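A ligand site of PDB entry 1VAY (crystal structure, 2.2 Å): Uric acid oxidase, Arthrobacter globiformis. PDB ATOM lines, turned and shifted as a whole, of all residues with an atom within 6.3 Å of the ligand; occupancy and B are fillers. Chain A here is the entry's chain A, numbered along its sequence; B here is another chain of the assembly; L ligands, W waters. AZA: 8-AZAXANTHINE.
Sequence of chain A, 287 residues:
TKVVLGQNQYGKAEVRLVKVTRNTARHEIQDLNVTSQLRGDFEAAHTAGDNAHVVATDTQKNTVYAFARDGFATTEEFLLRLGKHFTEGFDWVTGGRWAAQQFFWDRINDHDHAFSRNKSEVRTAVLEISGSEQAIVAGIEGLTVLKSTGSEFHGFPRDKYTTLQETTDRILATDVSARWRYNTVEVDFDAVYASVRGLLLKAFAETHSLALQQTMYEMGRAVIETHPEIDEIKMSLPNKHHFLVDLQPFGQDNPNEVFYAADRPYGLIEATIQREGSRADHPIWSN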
ATOM      1  N   GLU A 152     -20.965 -24.283  -9.243  1.00  0.00           N
ATOM      2  CA  GLU A 152     -20.925 -22.852  -9.495  1.00  0.00           C
ATOM      3  C   GLU A 152     -19.545 -22.304  -9.137  1.00  0.00           C
ATOM      4  O   GLU A 152     -18.766 -22.967  -8.457  1.00  0.00           O
ATOM      5  CB  GLU A 152     -21.954 -22.133  -8.628  1.00  0.00           C
ATOM      6  CG  GLU A 152     -23.395 -22.592  -8.798  1.00  0.00           C
ATOM      7  CD  GLU A 152     -24.374 -21.780  -7.943  1.00  0.00           C
ATOM      8  OE1 GLU A 152     -24.274 -20.534  -7.946  1.00  0.00           O
ATOM      9  OE2 GLU A 152     -25.238 -22.391  -7.273  1.00  0.00           O
ATOM     10  N   PHE A 153     -19.267 -21.097  -9.613  1.00  0.00           N
ATOM     11  CA  PHE A 153     -18.021 -20.402  -9.310  1.00  0.00           C
ATOM     12  C   PHE A 153     -18.208 -18.914  -9.564  1.00  0.00           C
ATOM     13  O   PHE A 153     -18.194 -18.454 -10.711  1.00  0.00           O
ATOM     14  CB  PHE A 153     -16.832 -20.889 -10.142  1.00  0.00           C
ATOM     15  CG  PHE A 153     -15.508 -20.348  -9.651  1.00  0.00           C
ATOM     16  CD1 PHE A 153     -15.090 -20.582  -8.342  1.00  0.00           C
ATOM     17  CD2 PHE A 153     -14.691 -19.593 -10.492  1.00  0.00           C
ATOM     18  CE1 PHE A 153     -13.872 -20.063  -7.868  1.00  0.00           C
ATOM     19  CE2 PHE A 153     -13.463 -19.066 -10.024  1.00  0.00           C
ATOM     20  CZ  PHE A 153     -13.052 -19.306  -8.718  1.00  0.00           C
ATOM     21  N   LEU A 164     -12.310 -14.120 -16.489  1.00  0.00           N
ATOM     22  CA  LEU A 164     -13.259 -15.201 -16.198  1.00  0.00           C
ATOM     23  C   LEU A 164     -14.591 -14.645 -15.716  1.00  0.00           C
ATOM     24  O   LEU A 164     -14.642 -13.836 -14.802  1.00  0.00           O
ATOM     25  CB  LEU A 164     -12.682 -16.134 -15.124  1.00  0.00           C
ATOM     26  CG  LEU A 164     -13.554 -17.315 -14.684  1.00  0.00           C
ATOM     27  CD1 LEU A 164     -13.768 -18.274 -15.862  1.00  0.00           C
ATOM     28  CD2 LEU A 164     -12.891 -18.033 -13.526  1.00  0.00           C
ATOM     29  N   ARG A 170     -22.075 -25.016 -14.313  1.00  0.00           N
ATOM     30  CA  ARG A 170     -20.911 -25.426 -15.078  1.00  0.00           C
ATOM     31  C   ARG A 170     -20.587 -26.888 -14.786  1.00  0.00           C
ATOM     32  O   ARG A 170     -21.105 -27.480 -13.841  1.00  0.00           O
ATOM     33  CB  ARG A 170     -19.702 -24.567 -14.710  1.00  0.00           C
ATOM     34  CG  ARG A 170     -19.190 -24.872 -13.304  1.00  0.00           C
ATOM     35  CD  ARG A 170     -17.841 -24.246 -13.031  1.00  0.00           C
ATOM     36  NE  ARG A 170     -17.340 -24.651 -11.720  1.00  0.00           N
ATOM     37  CZ  ARG A 170     -16.158 -24.309 -11.218  1.00  0.00           C
ATOM     38  NH1 ARG A 170     -15.334 -23.527 -11.909  1.00  0.00           N
ATOM     39  NH2 ARG A 170     -15.803 -24.752 -10.016  1.00  0.00           N
ATOM     40  N   LEU A 172     -18.032 -29.799 -13.542  1.00  0.00           N
ATOM     41  CA  LEU A 172     -16.911 -29.910 -12.619  1.00  0.00           C
ATOM     42  C   LEU A 172     -16.349 -31.308 -12.766  1.00  0.00           C
ATOM     43  O   LEU A 172     -16.979 -32.291 -12.371  1.00  0.00           O
ATOM     44  CB  LEU A 172     -17.357 -29.687 -11.163  1.00  0.00           C
ATOM     45  CG  LEU A 172     -16.211 -29.755 -10.145  1.00  0.00           C
ATOM     46  CD1 LEU A 172     -15.231 -28.616 -10.432  1.00  0.00           C
ATOM     47  CD2 LEU A 172     -16.746 -29.651  -8.726  1.00  0.00           C
ATOM     48  N   SER A 209     -21.486 -27.812  -5.337  1.00  0.00           N
ATOM     49  CA  SER A 209     -20.222 -27.085  -5.387  1.00  0.00           C
ATOM     50  C   SER A 209     -20.191 -25.611  -5.750  1.00  0.00           C
ATOM     51  O   SER A 209     -20.675 -25.206  -6.797  1.00  0.00           O
ATOM     52  CB  SER A 209     -19.260 -27.819  -6.324  1.00  0.00           C
ATOM     53  OG  SER A 209     -17.999 -27.192  -6.326  1.00  0.00           O
ATOM     54  N   LEU A 210     -19.601 -24.812  -4.855  1.00  0.00           N
ATOM     55  CA  LEU A 210     -19.443 -23.374  -5.080  1.00  0.00           C
ATOM     56  C   LEU A 210     -17.995 -23.131  -5.495  1.00  0.00           C
ATOM     57  O   LEU A 210     -17.615 -22.031  -5.904  1.00  0.00           O
ATOM     58  CB  LEU A 210     -19.778 -22.579  -3.814  1.00  0.00           C
ATOM     59  CG  LEU A 210     -21.245 -22.573  -3.381  1.00  0.00           C
ATOM     60  CD1 LEU A 210     -21.447 -21.634  -2.198  1.00  0.00           C
ATOM     61  CD2 LEU A 210     -22.108 -22.112  -4.541  1.00  0.00           C
ATOM     62  N   ALA A 211     -17.186 -24.185  -5.397  1.00  0.00           N
ATOM     63  CA  ALA A 211     -15.778 -24.151  -5.773  1.00  0.00           C
ATOM     64  C   ALA A 211     -15.132 -25.519  -5.561  1.00  0.00           C
ATOM     65  O   ALA A 211     -15.513 -26.258  -4.645  1.00  0.00           O
ATOM     66  CB  ALA A 211     -15.045 -23.084  -4.956  1.00  0.00           C
ATOM     67  N   LEU A 212     -14.152 -25.861  -6.397  1.00  0.00           N
ATOM     68  CA  LEU A 212     -13.492 -27.150  -6.268  1.00  0.00           C
ATOM     69  C   LEU A 212     -12.911 -27.243  -4.849  1.00  0.00           C
ATOM     70  O   LEU A 212     -12.849 -28.317  -4.263  1.00  0.00           O
ATOM     71  CB  LEU A 212     -12.373 -27.304  -7.302  1.00  0.00           C
ATOM     72  CG  LEU A 212     -12.117 -28.728  -7.832  1.00  0.00           C
ATOM     73  CD1 LEU A 212     -10.805 -28.749  -8.609  1.00  0.00           C
ATOM     74  CD2 LEU A 212     -12.066 -29.717  -6.687  1.00  0.00           C
ATOM     75  N   GLN A 213     -12.499 -26.100  -4.306  1.00  0.00           N
ATOM     76  CA  GLN A 213     -11.957 -26.023  -2.961  1.00  0.00           C
ATOM     77  C   GLN A 213     -13.009 -26.524  -1.951  1.00  0.00           C
ATOM     78  O   GLN A 213     -12.706 -27.360  -1.109  1.00  0.00           O
ATOM     79  CB  GLN A 213     -11.559 -24.575  -2.611  1.00  0.00           C
ATOM     80  CG  GLN A 213     -10.227 -24.102  -3.227  1.00  0.00           C
ATOM     81  CD  GLN A 213     -10.395 -23.552  -4.645  1.00  0.00           C
ATOM     82  OE1 GLN A 213     -11.247 -23.998  -5.396  1.00  0.00           O
ATOM     83  NE2 GLN A 213      -9.548 -22.591  -5.000  1.00  0.00           N
ATOM     84  N   ASN A 239      -8.657 -29.247 -12.011  1.00  0.00           N
ATOM     85  CA  ASN A 239      -9.961 -28.789 -12.465  1.00  0.00           C
ATOM     86  C   ASN A 239      -9.856 -28.975 -13.984  1.00  0.00           C
ATOM     87  O   ASN A 239      -9.347 -28.113 -14.698  1.00  0.00           O
ATOM     88  CB  ASN A 239     -10.144 -27.312 -12.071  1.00  0.00           C
ATOM     89  CG  ASN A 239     -11.548 -26.817 -12.288  1.00  0.00           C
ATOM     90  OD1 ASN A 239     -12.497 -27.591 -12.455  1.00  0.00           O
ATOM     91  ND2 ASN A 239     -11.712 -25.494 -12.265  1.00  0.00           N
ATOM     92  N   HIS A 241     -10.905 -28.545 -17.124  1.00  0.00           N
ATOM     93  CA  HIS A 241     -11.826 -27.669 -17.801  1.00  0.00           C
ATOM     94  C   HIS A 241     -12.522 -28.221 -19.030  1.00  0.00           C
ATOM     95  O   HIS A 241     -11.902 -28.841 -19.901  1.00  0.00           O
ATOM     96  CB  HIS A 241     -11.131 -26.350 -18.129  1.00  0.00           C
ATOM     97  CG  HIS A 241     -10.655 -25.623 -16.911  1.00  0.00           C
ATOM     98  ND1 HIS A 241      -9.369 -25.730 -16.433  1.00  0.00           N
ATOM     99  CD2 HIS A 241     -11.322 -24.851 -16.014  1.00  0.00           C
ATOM    100  CE1 HIS A 241      -9.264 -25.066 -15.292  1.00  0.00           C
ATOM    101  NE2 HIS A 241     -10.438 -24.532 -15.016  1.00  0.00           N
ATOM    102  N   ILE A 269      -6.074 -27.661  -7.596  1.00  0.00           N
ATOM    103  CA  ILE A 269      -6.476 -27.298  -6.250  1.00  0.00           C
ATOM    104  C   ILE A 269      -6.079 -28.448  -5.333  1.00  0.00           C
ATOM    105  O   ILE A 269      -6.476 -29.592  -5.558  1.00  0.00           O
ATOM    106  CB  ILE A 269      -8.018 -27.043  -6.206  1.00  0.00           C
ATOM    107  CG1 ILE A 269      -8.331 -25.685  -6.836  1.00  0.00           C
ATOM    108  CG2 ILE A 269      -8.538 -27.079  -4.778  1.00  0.00           C
ATOM    109  CD1 ILE A 269      -7.869 -25.509  -8.278  1.00  0.00           C
ATOM    110  N   TYR B  10      -3.321 -23.665  -4.470  1.00  0.00           N
ATOM    111  CA  TYR B  10      -4.119 -23.808  -5.686  1.00  0.00           C
ATOM    112  C   TYR B  10      -3.629 -22.825  -6.740  1.00  0.00           C
ATOM    113  O   TYR B  10      -3.032 -21.801  -6.409  1.00  0.00           O
ATOM    114  CB  TYR B  10      -5.590 -23.514  -5.382  1.00  0.00           C
ATOM    115  CG  TYR B  10      -5.913 -22.042  -5.455  1.00  0.00           C
ATOM    116  CD1 TYR B  10      -5.484 -21.172  -4.461  1.00  0.00           C
ATOM    117  CD2 TYR B  10      -6.574 -21.505  -6.564  1.00  0.00           C
ATOM    118  CE1 TYR B  10      -5.698 -19.806  -4.561  1.00  0.00           C
ATOM    119  CE2 TYR B  10      -6.790 -20.126  -6.683  1.00  0.00           C
ATOM    120  CZ  TYR B  10      -6.345 -19.283  -5.670  1.00  0.00           C
ATOM    121  OH  TYR B  10      -6.547 -17.918  -5.788  1.00  0.00           O
ATOM    122  N   GLY B  11      -3.913 -23.134  -8.013  1.00  0.00           N
ATOM    123  CA  GLY B  11      -3.505 -22.262  -9.101  1.00  0.00           C
ATOM    124  C   GLY B  11      -3.686 -22.926 -10.459  1.00  0.00           C
ATOM    125  O   GLY B  11      -4.416 -23.904 -10.591  1.00  0.00           O
ATOM    126  N   LYS B  12      -3.016 -22.397 -11.471  1.00  0.00           N
ATOM    127  CA  LYS B  12      -3.118 -22.966 -12.812  1.00  0.00           C
ATOM    128  C   LYS B  12      -1.847 -23.719 -13.160  1.00  0.00           C
ATOM    129  O   LYS B  12      -0.757 -23.138 -13.185  1.00  0.00           O
ATOM    130  CB  LYS B  12      -3.352 -21.872 -13.856  1.00  0.00           C
ATOM    131  CG  LYS B  12      -3.749 -22.427 -15.219  1.00  0.00           C
ATOM    132  CD  LYS B  12      -5.165 -23.037 -15.195  1.00  0.00           C
ATOM    133  CE  LYS B  12      -6.236 -21.955 -15.129  1.00  0.00           C
ATOM    134  NZ  LYS B  12      -7.639 -22.481 -15.090  1.00  0.00           N
ATOM    135  N   ASN B  51     -15.519 -17.324  -2.218  1.00  0.00           N
ATOM    136  CA  ASN B  51     -14.384 -17.103  -3.115  1.00  0.00           C
ATOM    137  C   ASN B  51     -13.787 -15.699  -3.158  1.00  0.00           C
ATOM    138  O   ASN B  51     -13.002 -15.376  -4.060  1.00  0.00           O
ATOM    139  CB  ASN B  51     -14.774 -17.512  -4.534  1.00  0.00           C
ATOM    140  CG  ASN B  51     -15.280 -18.942  -4.599  1.00  0.00           C
ATOM    141  OD1 ASN B  51     -14.565 -19.882  -4.251  1.00  0.00           O
ATOM    142  ND2 ASN B  51     -16.520 -19.112  -5.040  1.00  0.00           N
ATOM    143  N   VAL B  54     -10.224 -15.997  -3.538  1.00  0.00           N
ATOM    144  CA  VAL B  54      -9.763 -16.815  -4.663  1.00  0.00           C
ATOM    145  C   VAL B  54      -9.398 -16.095  -5.967  1.00  0.00           C
ATOM    146  O   VAL B  54     -10.260 -15.861  -6.809  1.00  0.00           O
ATOM    147  CB  VAL B  54     -10.803 -17.928  -4.981  1.00  0.00           C
ATOM    148  CG1 VAL B  54     -10.283 -18.828  -6.088  1.00  0.00           C
ATOM    149  CG2 VAL B  54     -11.093 -18.759  -3.716  1.00  0.00           C
ATOM    150  N   VAL B  55      -8.124 -15.730  -6.112  1.00  0.00           N
ATOM    151  CA  VAL B  55      -7.658 -15.117  -7.348  1.00  0.00           C
ATOM    152  C   VAL B  55      -7.740 -16.291  -8.348  1.00  0.00           C
ATOM    153  O   VAL B  55      -6.965 -17.239  -8.275  1.00  0.00           O
ATOM    154  CB  VAL B  55      -6.196 -14.639  -7.220  1.00  0.00           C
ATOM    155  CG1 VAL B  55      -5.657 -14.212  -8.571  1.00  0.00           C
ATOM    156  CG2 VAL B  55      -6.120 -13.473  -6.247  1.00  0.00           C
ATOM    157  N   ALA B  56      -8.684 -16.213  -9.279  1.00  0.00           N
ATOM    158  CA  ALA B  56      -8.907 -17.300 -10.245  1.00  0.00           C
ATOM    159  C   ALA B  56      -7.669 -17.899 -10.886  1.00  0.00           C
ATOM    160  O   ALA B  56      -6.725 -17.181 -11.244  1.00  0.00           O
ATOM    161  CB  ALA B  56      -9.872 -16.853 -11.311  1.00  0.00           C
ATOM    162  N   THR B  57      -7.690 -19.216 -11.052  1.00  0.00           N
ATOM    163  CA  THR B  57      -6.580 -19.902 -11.691  1.00  0.00           C
ATOM    164  C   THR B  57      -6.530 -19.389 -13.127  1.00  0.00           C
ATOM    165  O   THR B  57      -5.461 -19.307 -13.746  1.00  0.00           O
ATOM    166  CB  THR B  57      -6.770 -21.452 -11.690  1.00  0.00           C
ATOM    167  OG1 THR B  57      -7.855 -21.811 -12.566  1.00  0.00           O
ATOM    168  CG2 THR B  57      -7.077 -21.940 -10.284  1.00  0.00           C
ATOM    169  N   ASP B  58      -7.696 -18.993 -13.653  1.00  0.00           N
ATOM    170  CA  ASP B  58      -7.765 -18.454 -15.010  1.00  0.00           C
ATOM    171  C   ASP B  58      -7.014 -17.124 -15.080  1.00  0.00           C
ATOM    172  O   ASP B  58      -6.379 -16.814 -16.075  1.00  0.00           O
ATOM    173  CB  ASP B  58      -9.212 -18.236 -15.433  1.00  0.00           C
ATOM    174  CG  ASP B  58      -9.325 -17.817 -16.901  1.00  0.00           C
ATOM    175  OD1 ASP B  58      -9.215 -18.707 -17.776  1.00  0.00           O
ATOM    176  OD2 ASP B  58      -9.500 -16.616 -17.174  1.00  0.00           O
ATOM    177  N   THR B  59      -7.088 -16.344 -13.996  1.00  0.00           N
ATOM    178  CA  THR B  59      -6.403 -15.061 -13.926  1.00  0.00           C
ATOM    179  C   THR B  59      -4.899 -15.279 -13.864  1.00  0.00           C
ATOM    180  O   THR B  59      -4.128 -14.606 -14.536  1.00  0.00           O
ATOM    181  CB  THR B  59      -6.853 -14.255 -12.693  1.00  0.00           C
ATOM    182  OG1 THR B  59      -8.280 -14.086 -12.723  1.00  0.00           O
ATOM    183  CG2 THR B  59      -6.199 -12.877 -12.683  1.00  0.00           C
HETATM  184  N1  AZA L   1     -11.666 -22.835  -8.122  1.00  0.00           N
HETATM  185  C2  AZA L   1     -12.780 -23.230  -8.833  1.00  0.00           C
HETATM  186  O2  AZA L   1     -13.592 -23.996  -8.350  1.00  0.00           O
HETATM  187  N3  AZA L   1     -12.961 -22.758 -10.092  1.00  0.00           N
HETATM  188  C4  AZA L   1     -12.087 -21.919 -10.622  1.00  0.00           C
HETATM  189  C5  AZA L   1     -10.965 -21.516  -9.939  1.00  0.00           C
HETATM  190  C6  AZA L   1     -10.690 -21.989  -8.576  1.00  0.00           C
HETATM  191  O6  AZA L   1      -9.727 -21.703  -7.865  1.00  0.00           O
HETATM  192  N7  AZA L   1     -10.274 -20.687 -10.724  1.00  0.00           N
HETATM  193  N8  AZA L   1     -11.019 -20.632 -11.848  1.00  0.00           N
HETATM  194  N9  AZA L   1     -12.130 -21.375 -11.819  1.00  0.00           N
HETATM  195  O   HOH W   1      -9.496 -23.936 -11.538  1.00  0.00           O
HETATM  196  O   HOH W   2     -13.343 -21.774 -14.258  1.00  0.00           O
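An oxygen (O2) of the ligand lies within hydrogen-bond range of the backbone NH of Leu 212 (2.8 Å).
The guanidinium group (NH2) of Arg 170 is in hydrogen-bond range of an oxygen (O2) of the ligand (2.9 Å).
The backbone NH (N) of Thr 57 of chain B sits at hydrogen-bond distance from a nitrogen (N7) of the ligand (3.0 Å).
OG1 of Thr 57 of chain B is in hydrogen-bond range of N7 of the ligand, at 3.2 Å.
OE1 of Gln 213 sits at hydrogen-bond distance from N1 of the ligand.
Phe 153 touches the ligand.
CD2 of Leu 164 touches N8 of the ligand, 3.6 Å away.
Ala 211 touches the ligand (CA to O2, 3.4 Å).
Asn 239 touches the ligand (ND2 to N3, 3.7 Å).
Tyr 10 of chain B touches the ligand.
Val 54 of chain B touches the ligand (CG1 to O6, 3.4 Å).
Ala 56 of chain B touches the ligand.
11 residues have an atom within 4 Å of the ligand: Phe 153, Leu 164, Arg 170, Ala 211, Leu 212, Gln 213, Asn 239, Tyr 10 of chain B, Val 54 of chain B, Ala 56 of chain B and Thr 57 of chain B.
Water W1 lies within hydrogen-bond range of the side-chain amide nitrogen (ND2) of Asn 239 (2.8 Å), the side-chain hydroxyl (OG1) of Thr 57 of chain B (2.9 Å) and a nitrogen (N7) of the ligand (3.4 Å).
NZ of Lys 12 of chain B lies within hydrogen-bond range of OG1 of Thr 57 of chain B, at 2.6 Å.
O of Ala 211 lies within hydrogen-bond range of OG of Ser 209.
The side-chain hydroxyl of Tyr 10 of chain B is in hydrogen-bond range of the backbone carbonyl oxygen of Val 55 of chain B, 2.6 Å away.
The backbone carbonyl oxygen of Asn 239 is in hydrogen-bond range of a ring nitrogen (ND1) of His 241, 2.9 Å away.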
